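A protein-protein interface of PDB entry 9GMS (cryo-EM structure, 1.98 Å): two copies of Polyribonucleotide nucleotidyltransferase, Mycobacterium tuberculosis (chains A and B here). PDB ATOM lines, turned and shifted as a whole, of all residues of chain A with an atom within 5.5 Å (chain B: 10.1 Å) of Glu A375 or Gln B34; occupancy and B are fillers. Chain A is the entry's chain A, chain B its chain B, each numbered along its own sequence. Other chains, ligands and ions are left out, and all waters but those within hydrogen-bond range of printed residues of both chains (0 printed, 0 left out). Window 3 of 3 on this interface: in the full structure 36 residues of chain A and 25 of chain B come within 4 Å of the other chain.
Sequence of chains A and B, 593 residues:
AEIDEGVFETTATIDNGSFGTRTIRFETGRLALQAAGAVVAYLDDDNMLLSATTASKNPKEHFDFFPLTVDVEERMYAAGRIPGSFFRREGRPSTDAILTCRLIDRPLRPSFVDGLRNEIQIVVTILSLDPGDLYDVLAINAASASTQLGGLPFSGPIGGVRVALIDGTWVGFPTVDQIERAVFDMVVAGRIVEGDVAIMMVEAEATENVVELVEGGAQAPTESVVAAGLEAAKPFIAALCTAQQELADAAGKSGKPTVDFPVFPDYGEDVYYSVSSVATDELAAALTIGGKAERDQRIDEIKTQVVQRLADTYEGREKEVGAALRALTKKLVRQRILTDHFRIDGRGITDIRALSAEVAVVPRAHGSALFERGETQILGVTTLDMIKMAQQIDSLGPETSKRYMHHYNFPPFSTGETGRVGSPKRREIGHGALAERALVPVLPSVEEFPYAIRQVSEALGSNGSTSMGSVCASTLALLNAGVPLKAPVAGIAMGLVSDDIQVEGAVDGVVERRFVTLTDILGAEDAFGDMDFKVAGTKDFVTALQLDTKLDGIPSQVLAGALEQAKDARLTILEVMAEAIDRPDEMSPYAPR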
ATOM      1  N   LYS A 292       5.528  -7.630  11.412  1.00  0.00           N
ATOM      2  CA  LYS A 292       5.240  -6.998  10.126  1.00  0.00           C
ATOM      3  C   LYS A 292       6.489  -6.661   9.324  1.00  0.00           C
ATOM      4  O   LYS A 292       6.991  -7.503   8.570  1.00  0.00           O
ATOM      5  CB  LYS A 292       4.426  -5.725  10.327  1.00  0.00           C
ATOM      6  CG  LYS A 292       2.983  -5.971  10.672  1.00  0.00           C
ATOM      7  CD  LYS A 292       2.197  -6.496   9.479  1.00  0.00           C
ATOM      8  CE  LYS A 292       2.135  -5.489   8.347  1.00  0.00           C
ATOM      9  NZ  LYS A 292       1.162  -5.889   7.303  1.00  0.00           N
ATOM     10  N   ARG A 353      -8.746  -6.725  17.278  1.00  0.00           N
ATOM     11  CA  ARG A 353      -7.672  -5.757  17.116  1.00  0.00           C
ATOM     12  C   ARG A 353      -8.027  -4.443  17.812  1.00  0.00           C
ATOM     13  O   ARG A 353      -9.175  -4.195  18.183  1.00  0.00           O
ATOM     14  CB  ARG A 353      -7.389  -5.519  15.634  1.00  0.00           C
ATOM     15  CG  ARG A 353      -6.779  -6.714  14.927  1.00  0.00           C
ATOM     16  CD  ARG A 353      -6.630  -6.488  13.433  1.00  0.00           C
ATOM     17  NE  ARG A 353      -7.885  -6.651  12.709  1.00  0.00           N
ATOM     18  CZ  ARG A 353      -8.028  -6.454  11.406  1.00  0.00           C
ATOM     19  NH1 ARG A 353      -7.023  -6.039  10.655  1.00  0.00           N
ATOM     20  NH2 ARG A 353      -9.212  -6.671  10.843  1.00  0.00           N
ATOM     21  N   ARG A 373      -9.861  -0.055  13.142  1.00  0.00           N
ATOM     22  CA  ARG A 373      -9.720  -1.378  13.741  1.00  0.00           C
ATOM     23  C   ARG A 373      -8.385  -1.939  13.265  1.00  0.00           C
ATOM     24  O   ARG A 373      -8.282  -2.489  12.166  1.00  0.00           O
ATOM     25  CB  ARG A 373     -10.884  -2.280  13.359  1.00  0.00           C
ATOM     26  CG  ARG A 373     -10.918  -3.607  14.087  1.00  0.00           C
ATOM     27  CD  ARG A 373     -12.197  -4.347  13.769  1.00  0.00           C
ATOM     28  NE  ARG A 373     -12.360  -4.482  12.328  1.00  0.00           N
ATOM     29  CZ  ARG A 373     -13.519  -4.439  11.689  1.00  0.00           C
ATOM     30  NH1 ARG A 373     -14.661  -4.272  12.333  1.00  0.00           N
ATOM     31  NH2 ARG A 373     -13.531  -4.556  10.366  1.00  0.00           N
ATOM     32  N   GLY A 374      -7.352  -1.724  14.070  1.00  0.00           N
ATOM     33  CA  GLY A 374      -6.055  -2.325  13.857  1.00  0.00           C
ATOM     34  C   GLY A 374      -5.309  -1.701  12.705  1.00  0.00           C
ATOM     35  O   GLY A 374      -4.338  -0.968  12.894  1.00  0.00           O
ATOM     36  N   GLU A 375      -5.771  -1.978  11.501  1.00  0.00           N
ATOM     37  CA  GLU A 375      -5.186  -1.406  10.302  1.00  0.00           C
ATOM     38  C   GLU A 375      -6.234  -1.096   9.248  1.00  0.00           C
ATOM     39  O   GLU A 375      -5.879  -0.583   8.185  1.00  0.00           O
ATOM     40  CB  GLU A 375      -4.127  -2.353   9.735  1.00  0.00           C
ATOM     41  CG  GLU A 375      -3.040  -1.662   8.964  1.00  0.00           C
ATOM     42  CD  GLU A 375      -1.829  -2.544   8.766  1.00  0.00           C
ATOM     43  OE1 GLU A 375      -1.606  -3.442   9.604  1.00  0.00           O
ATOM     44  OE2 GLU A 375      -1.099  -2.347   7.773  1.00  0.00           O
ATOM     45  N   THR A 376      -7.501  -1.400   9.502  1.00  0.00           N
ATOM     46  CA  THR A 376      -8.590  -0.975   8.642  1.00  0.00           C
ATOM     47  C   THR A 376      -9.107   0.371   9.134  1.00  0.00           C
ATOM     48  O   THR A 376      -9.402   0.532  10.322  1.00  0.00           O
ATOM     49  CB  THR A 376      -9.697  -2.030   8.632  1.00  0.00           C
ATOM     50  OG1 THR A 376      -9.233  -3.192   7.938  1.00  0.00           O
ATOM     51  CG2 THR A 376     -10.947  -1.509   7.959  1.00  0.00           C
ATOM     52  N   GLN A 377      -9.194   1.338   8.221  1.00  0.00           N
ATOM     53  CA  GLN A 377      -9.523   2.720   8.557  1.00  0.00           C
ATOM     54  C   GLN A 377     -10.583   3.226   7.593  1.00  0.00           C
ATOM     55  O   GLN A 377     -10.344   3.251   6.378  1.00  0.00           O
ATOM     56  CB  GLN A 377      -8.278   3.609   8.486  1.00  0.00           C
ATOM     57  CG  GLN A 377      -8.522   5.062   8.841  1.00  0.00           C
ATOM     58  CD  GLN A 377      -7.263   5.901   8.753  1.00  0.00           C
ATOM     59  OE1 GLN A 377      -6.775   6.194   7.668  1.00  0.00           O
ATOM     60  NE2 GLN A 377      -6.731   6.288   9.900  1.00  0.00           N
ATOM     61  N   PHE A 413      -4.830   3.401  -3.470  1.00  0.00           N
ATOM     62  CA  PHE A 413      -3.825   3.614  -2.432  1.00  0.00           C
ATOM     63  C   PHE A 413      -4.229   3.022  -1.087  1.00  0.00           C
ATOM     64  O   PHE A 413      -3.419   3.039  -0.157  1.00  0.00           O
ATOM     65  CB  PHE A 413      -3.511   5.111  -2.282  1.00  0.00           C
ATOM     66  CG  PHE A 413      -4.663   5.953  -1.792  1.00  0.00           C
ATOM     67  CD1 PHE A 413      -4.966   6.030  -0.445  1.00  0.00           C
ATOM     68  CD2 PHE A 413      -5.414   6.703  -2.679  1.00  0.00           C
ATOM     69  CE1 PHE A 413      -6.013   6.809   0.001  1.00  0.00           C
ATOM     70  CE2 PHE A 413      -6.461   7.487  -2.235  1.00  0.00           C
ATOM     71  CZ  PHE A 413      -6.759   7.542  -0.895  1.00  0.00           C
ATOM     72  N   SER A 414      -5.451   2.498  -0.968  1.00  0.00           N
ATOM     73  CA  SER A 414      -5.899   1.881   0.275  1.00  0.00           C
ATOM     74  C   SER A 414      -5.031   0.691   0.670  1.00  0.00           C
ATOM     75  O   SER A 414      -4.889   0.401   1.862  1.00  0.00           O
ATOM     76  CB  SER A 414      -7.360   1.455   0.125  1.00  0.00           C
ATOM     77  OG  SER A 414      -7.912   1.020   1.350  1.00  0.00           O
ATOM     78  N   THR A 415      -4.455  -0.016  -0.304  1.00  0.00           N
ATOM     79  CA  THR A 415      -3.511  -1.097  -0.037  1.00  0.00           C
ATOM     80  C   THR A 415      -2.118  -0.797  -0.576  1.00  0.00           C
ATOM     81  O   THR A 415      -1.272  -1.693  -0.603  1.00  0.00           O
ATOM     82  CB  THR A 415      -4.008  -2.424  -0.627  1.00  0.00           C
ATOM     83  OG1 THR A 415      -4.215  -2.281  -2.037  1.00  0.00           O
ATOM     84  CG2 THR A 415      -5.306  -2.869   0.023  1.00  0.00           C
ATOM     85  N   GLY A 416      -1.860   0.432  -1.017  1.00  0.00           N
ATOM     86  CA  GLY A 416      -0.551   0.789  -1.521  1.00  0.00           C
ATOM     87  C   GLY A 416      -0.314   0.488  -2.985  1.00  0.00           C
ATOM     88  O   GLY A 416       0.844   0.417  -3.401  1.00  0.00           O
ATOM     89  N   GLY A 461      -7.916   2.867   4.572  1.00  0.00           N
ATOM     90  CA  GLY A 461      -6.965   1.780   4.738  1.00  0.00           C
ATOM     91  C   GLY A 461      -7.639   0.429   4.848  1.00  0.00           C
ATOM     92  O   GLY A 461      -8.594   0.294   5.613  1.00  0.00           O
ATOM     93  N   SER A 462      -7.163  -0.578   4.116  1.00  0.00           N
ATOM     94  CA  SER A 462      -7.857  -1.857   4.005  1.00  0.00           C
ATOM     95  C   SER A 462      -6.934  -3.001   4.400  1.00  0.00           C
ATOM     96  O   SER A 462      -5.898  -3.214   3.766  1.00  0.00           O
ATOM     97  CB  SER A 462      -8.381  -2.072   2.581  1.00  0.00           C
ATOM     98  OG  SER A 462      -9.241  -1.018   2.190  1.00  0.00           O
ATOM     99  N   ASN A 463      -7.311  -3.729   5.449  1.00  0.00           N
ATOM    100  CA  ASN A 463      -6.666  -4.988   5.818  1.00  0.00           C
ATOM    101  C   ASN A 463      -7.702  -5.980   6.333  1.00  0.00           C
ATOM    102  O   ASN A 463      -7.514  -6.614   7.374  1.00  0.00           O
ATOM    103  CB  ASN A 463      -5.565  -4.765   6.854  1.00  0.00           C
ATOM    104  CG  ASN A 463      -4.616  -5.949   6.962  1.00  0.00           C
ATOM    105  OD1 ASN A 463      -4.535  -6.774   6.062  1.00  0.00           O
ATOM    106  ND2 ASN A 463      -3.887  -6.023   8.060  1.00  0.00           N
ATOM    107  N   GLY B  29       0.820  11.702   9.117  1.00  0.00           N
ATOM    108  CA  GLY B  29       0.933  10.629  10.079  1.00  0.00           C
ATOM    109  C   GLY B  29      -0.364  10.094  10.644  1.00  0.00           C
ATOM    110  O   GLY B  29      -0.324   9.356  11.632  1.00  0.00           O
ATOM    111  N   ARG B  30      -1.504  10.425  10.052  1.00  0.00           N
ATOM    112  CA  ARG B  30      -2.796  10.065  10.632  1.00  0.00           C
ATOM    113  C   ARG B  30      -3.741   9.366   9.661  1.00  0.00           C
ATOM    114  O   ARG B  30      -4.463   8.460  10.077  1.00  0.00           O
ATOM    115  CB  ARG B  30      -3.451  11.334  11.185  1.00  0.00           C
ATOM    116  CG  ARG B  30      -4.815  11.135  11.802  1.00  0.00           C
ATOM    117  CD  ARG B  30      -5.375  12.462  12.273  1.00  0.00           C
ATOM    118  NE  ARG B  30      -6.717  12.337  12.825  1.00  0.00           N
ATOM    119  CZ  ARG B  30      -7.401  13.339  13.362  1.00  0.00           C
ATOM    120  NH1 ARG B  30      -6.899  14.561  13.429  1.00  0.00           N
ATOM    121  NH2 ARG B  30      -8.616  13.108  13.850  1.00  0.00           N
ATOM    122  N   LEU B  31      -3.759   9.755   8.387  1.00  0.00           N
ATOM    123  CA  LEU B  31      -4.666   9.182   7.399  1.00  0.00           C
ATOM    124  C   LEU B  31      -3.879   8.503   6.285  1.00  0.00           C
ATOM    125  O   LEU B  31      -2.779   8.938   5.937  1.00  0.00           O
ATOM    126  CB  LEU B  31      -5.582  10.254   6.795  1.00  0.00           C
ATOM    127  CG  LEU B  31      -6.446  11.067   7.761  1.00  0.00           C
ATOM    128  CD1 LEU B  31      -7.348  12.014   6.997  1.00  0.00           C
ATOM    129  CD2 LEU B  31      -7.269  10.166   8.652  1.00  0.00           C
ATOM    130  N   ALA B  32      -4.448   7.426   5.740  1.00  0.00           N
ATOM    131  CA  ALA B  32      -3.913   6.731   4.566  1.00  0.00           C
ATOM    132  C   ALA B  32      -2.460   6.300   4.782  1.00  0.00           C
ATOM    133  O   ALA B  32      -1.546   6.705   4.065  1.00  0.00           O
ATOM    134  CB  ALA B  32      -4.046   7.603   3.314  1.00  0.00           C
ATOM    135  N   LEU B  33      -2.269   5.438   5.778  1.00  0.00           N
ATOM    136  CA  LEU B  33      -0.936   5.056   6.224  1.00  0.00           C
ATOM    137  C   LEU B  33      -0.281   3.982   5.363  1.00  0.00           C
ATOM    138  O   LEU B  33       0.905   3.705   5.564  1.00  0.00           O
ATOM    139  CB  LEU B  33      -1.002   4.576   7.673  1.00  0.00           C
ATOM    140  CG  LEU B  33      -1.594   5.579   8.668  1.00  0.00           C
ATOM    141  CD1 LEU B  33      -1.630   4.989  10.059  1.00  0.00           C
ATOM    142  CD2 LEU B  33      -0.818   6.880   8.669  1.00  0.00           C
ATOM    143  N   GLN B  34      -0.997   3.366   4.426  1.00  0.00           N
ATOM    144  CA  GLN B  34      -0.401   2.369   3.543  1.00  0.00           C
ATOM    145  C   GLN B  34       0.084   2.952   2.223  1.00  0.00           C
ATOM    146  O   GLN B  34       0.657   2.217   1.415  1.00  0.00           O
ATOM    147  CB  GLN B  34      -1.392   1.232   3.270  1.00  0.00           C
ATOM    148  CG  GLN B  34      -1.660   0.339   4.473  1.00  0.00           C
ATOM    149  CD  GLN B  34      -2.493  -0.881   4.129  1.00  0.00           C
ATOM    150  OE1 GLN B  34      -2.194  -1.603   3.181  1.00  0.00           O
ATOM    151  NE2 GLN B  34      -3.548  -1.115   4.899  1.00  0.00           N
ATOM    152  N   ALA B  35      -0.135   4.238   1.973  1.00  0.00           N
ATOM    153  CA  ALA B  35       0.426   4.878   0.796  1.00  0.00           C
ATOM    154  C   ALA B  35       1.908   5.168   1.009  1.00  0.00           C
ATOM    155  O   ALA B  35       2.413   5.154   2.132  1.00  0.00           O
ATOM    156  CB  ALA B  35      -0.319   6.172   0.478  1.00  0.00           C
ATOM    157  N   ALA B  36       2.612   5.430  -0.094  1.00  0.00           N
ATOM    158  CA  ALA B  36       4.011   5.828   0.021  1.00  0.00           C
ATOM    159  C   ALA B  36       4.143   7.157   0.756  1.00  0.00           C
ATOM    160  O   ALA B  36       5.033   7.319   1.595  1.00  0.00           O
ATOM    161  CB  ALA B  36       4.661   5.907  -1.359  1.00  0.00           C
ATOM    162  N   GLY B  37       3.271   8.113   0.462  1.00  0.00           N
ATOM    163  CA  GLY B  37       3.225   9.347   1.233  1.00  0.00           C
ATOM    164  C   GLY B  37       1.836   9.940   1.217  1.00  0.00           C
ATOM    165  O   GLY B  37       1.101   9.800   0.239  1.00  0.00           O
ATOM    166  N   ALA B  38       1.472  10.613   2.308  1.00  0.00           N
ATOM    167  CA  ALA B  38       0.135  11.187   2.421  1.00  0.00           C
ATOM    168  C   ALA B  38       0.170  12.435   3.293  1.00  0.00           C
ATOM    169  O   ALA B  38       0.846  12.457   4.322  1.00  0.00           O
ATOM    170  CB  ALA B  38      -0.857  10.174   2.995  1.00  0.00           C
ATOM    171  N   LEU B  50      -7.035  16.094   1.058  1.00  0.00           N
ATOM    172  CA  LEU B  50      -6.081  15.015   1.299  1.00  0.00           C
ATOM    173  C   LEU B  50      -5.377  14.635   0.005  1.00  0.00           C
ATOM    174  O   LEU B  50      -6.015  14.541  -1.046  1.00  0.00           O
ATOM    175  CB  LEU B  50      -6.777  13.769   1.882  1.00  0.00           C
ATOM    176  CG  LEU B  50      -5.985  12.451   1.920  1.00  0.00           C
ATOM    177  CD1 LEU B  50      -4.917  12.468   3.000  1.00  0.00           C
ATOM    178  CD2 LEU B  50      -6.909  11.264   2.107  1.00  0.00           C
ATOM    179  N   ALA B  52      -2.436  11.780  -1.630  1.00  0.00           N
ATOM    180  CA  ALA B  52      -1.725  10.521  -1.436  1.00  0.00           C
ATOM    181  C   ALA B  52      -0.943  10.151  -2.688  1.00  0.00           C
ATOM    182  O   ALA B  52      -1.443  10.297  -3.805  1.00  0.00           O
ATOM    183  CB  ALA B  52      -2.695   9.386  -1.087  1.00  0.00           C
ATOM    184  N   THR B  53       0.277   9.648  -2.492  1.00  0.00           N
ATOM    185  CA  THR B  53       1.182   9.262  -3.569  1.00  0.00           C
ATOM    186  C   THR B  53       1.682   7.841  -3.344  1.00  0.00           C
ATOM    187  O   THR B  53       2.098   7.494  -2.232  1.00  0.00           O
ATOM    188  CB  THR B  53       2.387  10.211  -3.652  1.00  0.00           C
ATOM    189  OG1 THR B  53       1.940  11.546  -3.908  1.00  0.00           O
ATOM    190  CG2 THR B  53       3.333   9.783  -4.754  1.00  0.00           C
ATOM    191  N   THR B  54       1.658   7.035  -4.412  1.00  0.00           N
ATOM    192  CA  THR B  54       2.133   5.655  -4.387  1.00  0.00           C
ATOM    193  C   THR B  54       2.928   5.359  -5.655  1.00  0.00           C
ATOM    194  O   THR B  54       2.844   6.079  -6.651  1.00  0.00           O
ATOM    195  CB  THR B  54       0.980   4.645  -4.266  1.00  0.00           C
ATOM    196  OG1 THR B  54       0.133   4.734  -5.414  1.00  0.00           O
ATOM    197  CG2 THR B  54       0.156   4.900  -3.028  1.00  0.00           C
ATOM    198  N   ALA B  55       3.697   4.269  -5.615  1.00  0.00           N
ATOM    199  CA  ALA B  55       4.534   3.848  -6.732  1.00  0.00           C
ATOM    200  C   ALA B  55       4.438   2.340  -6.915  1.00  0.00           C
ATOM    201  O   ALA B  55       4.294   1.592  -5.947  1.00  0.00           O
ATOM    202  CB  ALA B  55       5.997   4.242  -6.513  1.00  0.00           C
ATOM    203  N   GLY B 150       7.078  10.928   0.258  1.00  0.00           N
ATOM    204  CA  GLY B 150       7.082   9.551  -0.191  1.00  0.00           C
ATOM    205  C   GLY B 150       8.438   8.929  -0.449  1.00  0.00           C
ATOM    206  O   GLY B 150       8.503   7.740  -0.769  1.00  0.00           O
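The side-chain amide nitrogen of Gln A377 lies within hydrogen-bond range of the backbone carbonyl oxygen of Arg B30 (3.1 Å). The side-chain amide oxygen of Gln A377 sits at hydrogen-bond distance from the backbone NH of Ala B32, 3.3 Å away. O of Ser A462 lies within hydrogen-bond range of NE2 of Gln B34, 3.3 Å away.
The backbone NH (N) of Gln A377 sits at hydrogen-bond distance from the backbone carbonyl oxygen (O) of Gly A461 (2.9 Å). The side-chain hydroxyl (OG) of Ser A414 is in hydrogen-bond range of the side-chain hydroxyl (OG) of Ser A462 (2.6 Å).
Among the printed residues, merely in contact across the chains: Gly A416 with Gln B34, Thr A415 with Gln B34, Ser A414 with Gln B34, Gln A377 with Leu B31, Phe A413 with Thr B54, Phe A413 with Ala B32 and Glu A375 with Gln B34.
No residue of chain B comes within 4 Å of Gly A374. Glu A375 touches one residue of chain B. No residue of chain B comes within 4 Å of Thr A376. Printed residues of chain B within 4 Å of Phe A413: Ala B32 (3.9 Å) and Thr B54 (3.7 Å). Gly A416 touches just one residue of chain B: Gln B34. No residue of chain B comes within 4 Å of Gly A461. Asn A463 touches none of the printed residues of chain B. Printed residues of chain A within 4 Å of Arg B30: Gln A377 (3.1 Å). Of the printed residues of chain A, Ala B32 touches Gln A377 and Phe A413. Gln B34 touches just these residues of chain A: Glu A375, Ser A414, Thr A415, Gly A416 and Ser A462. The nearest residue of chain B that does not touch Glu A375 is Leu B33 (6.7 Å).
Of the 14 printed residues of chain A, 7 touch a printed residue of chain B. Hydrophobic or aromatic side chains of chain A that line the printed part of chain B: Phe A413. Of the 16 printed residues of chain B, 5 touch a printed residue of chain A. Hydrophobic or aromatic side chains of chain B that line the printed part of chain A: Ala B32. Among the printed residues, no Asp or Glu carboxylate lies within 4 Å of a Lys or Arg side-chain nitrogen of the other chain.
No position is printed for both chains. Of the 10 pairs that touch across the chains among the printed residues, none has its exchanged pair printed and touching as well.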
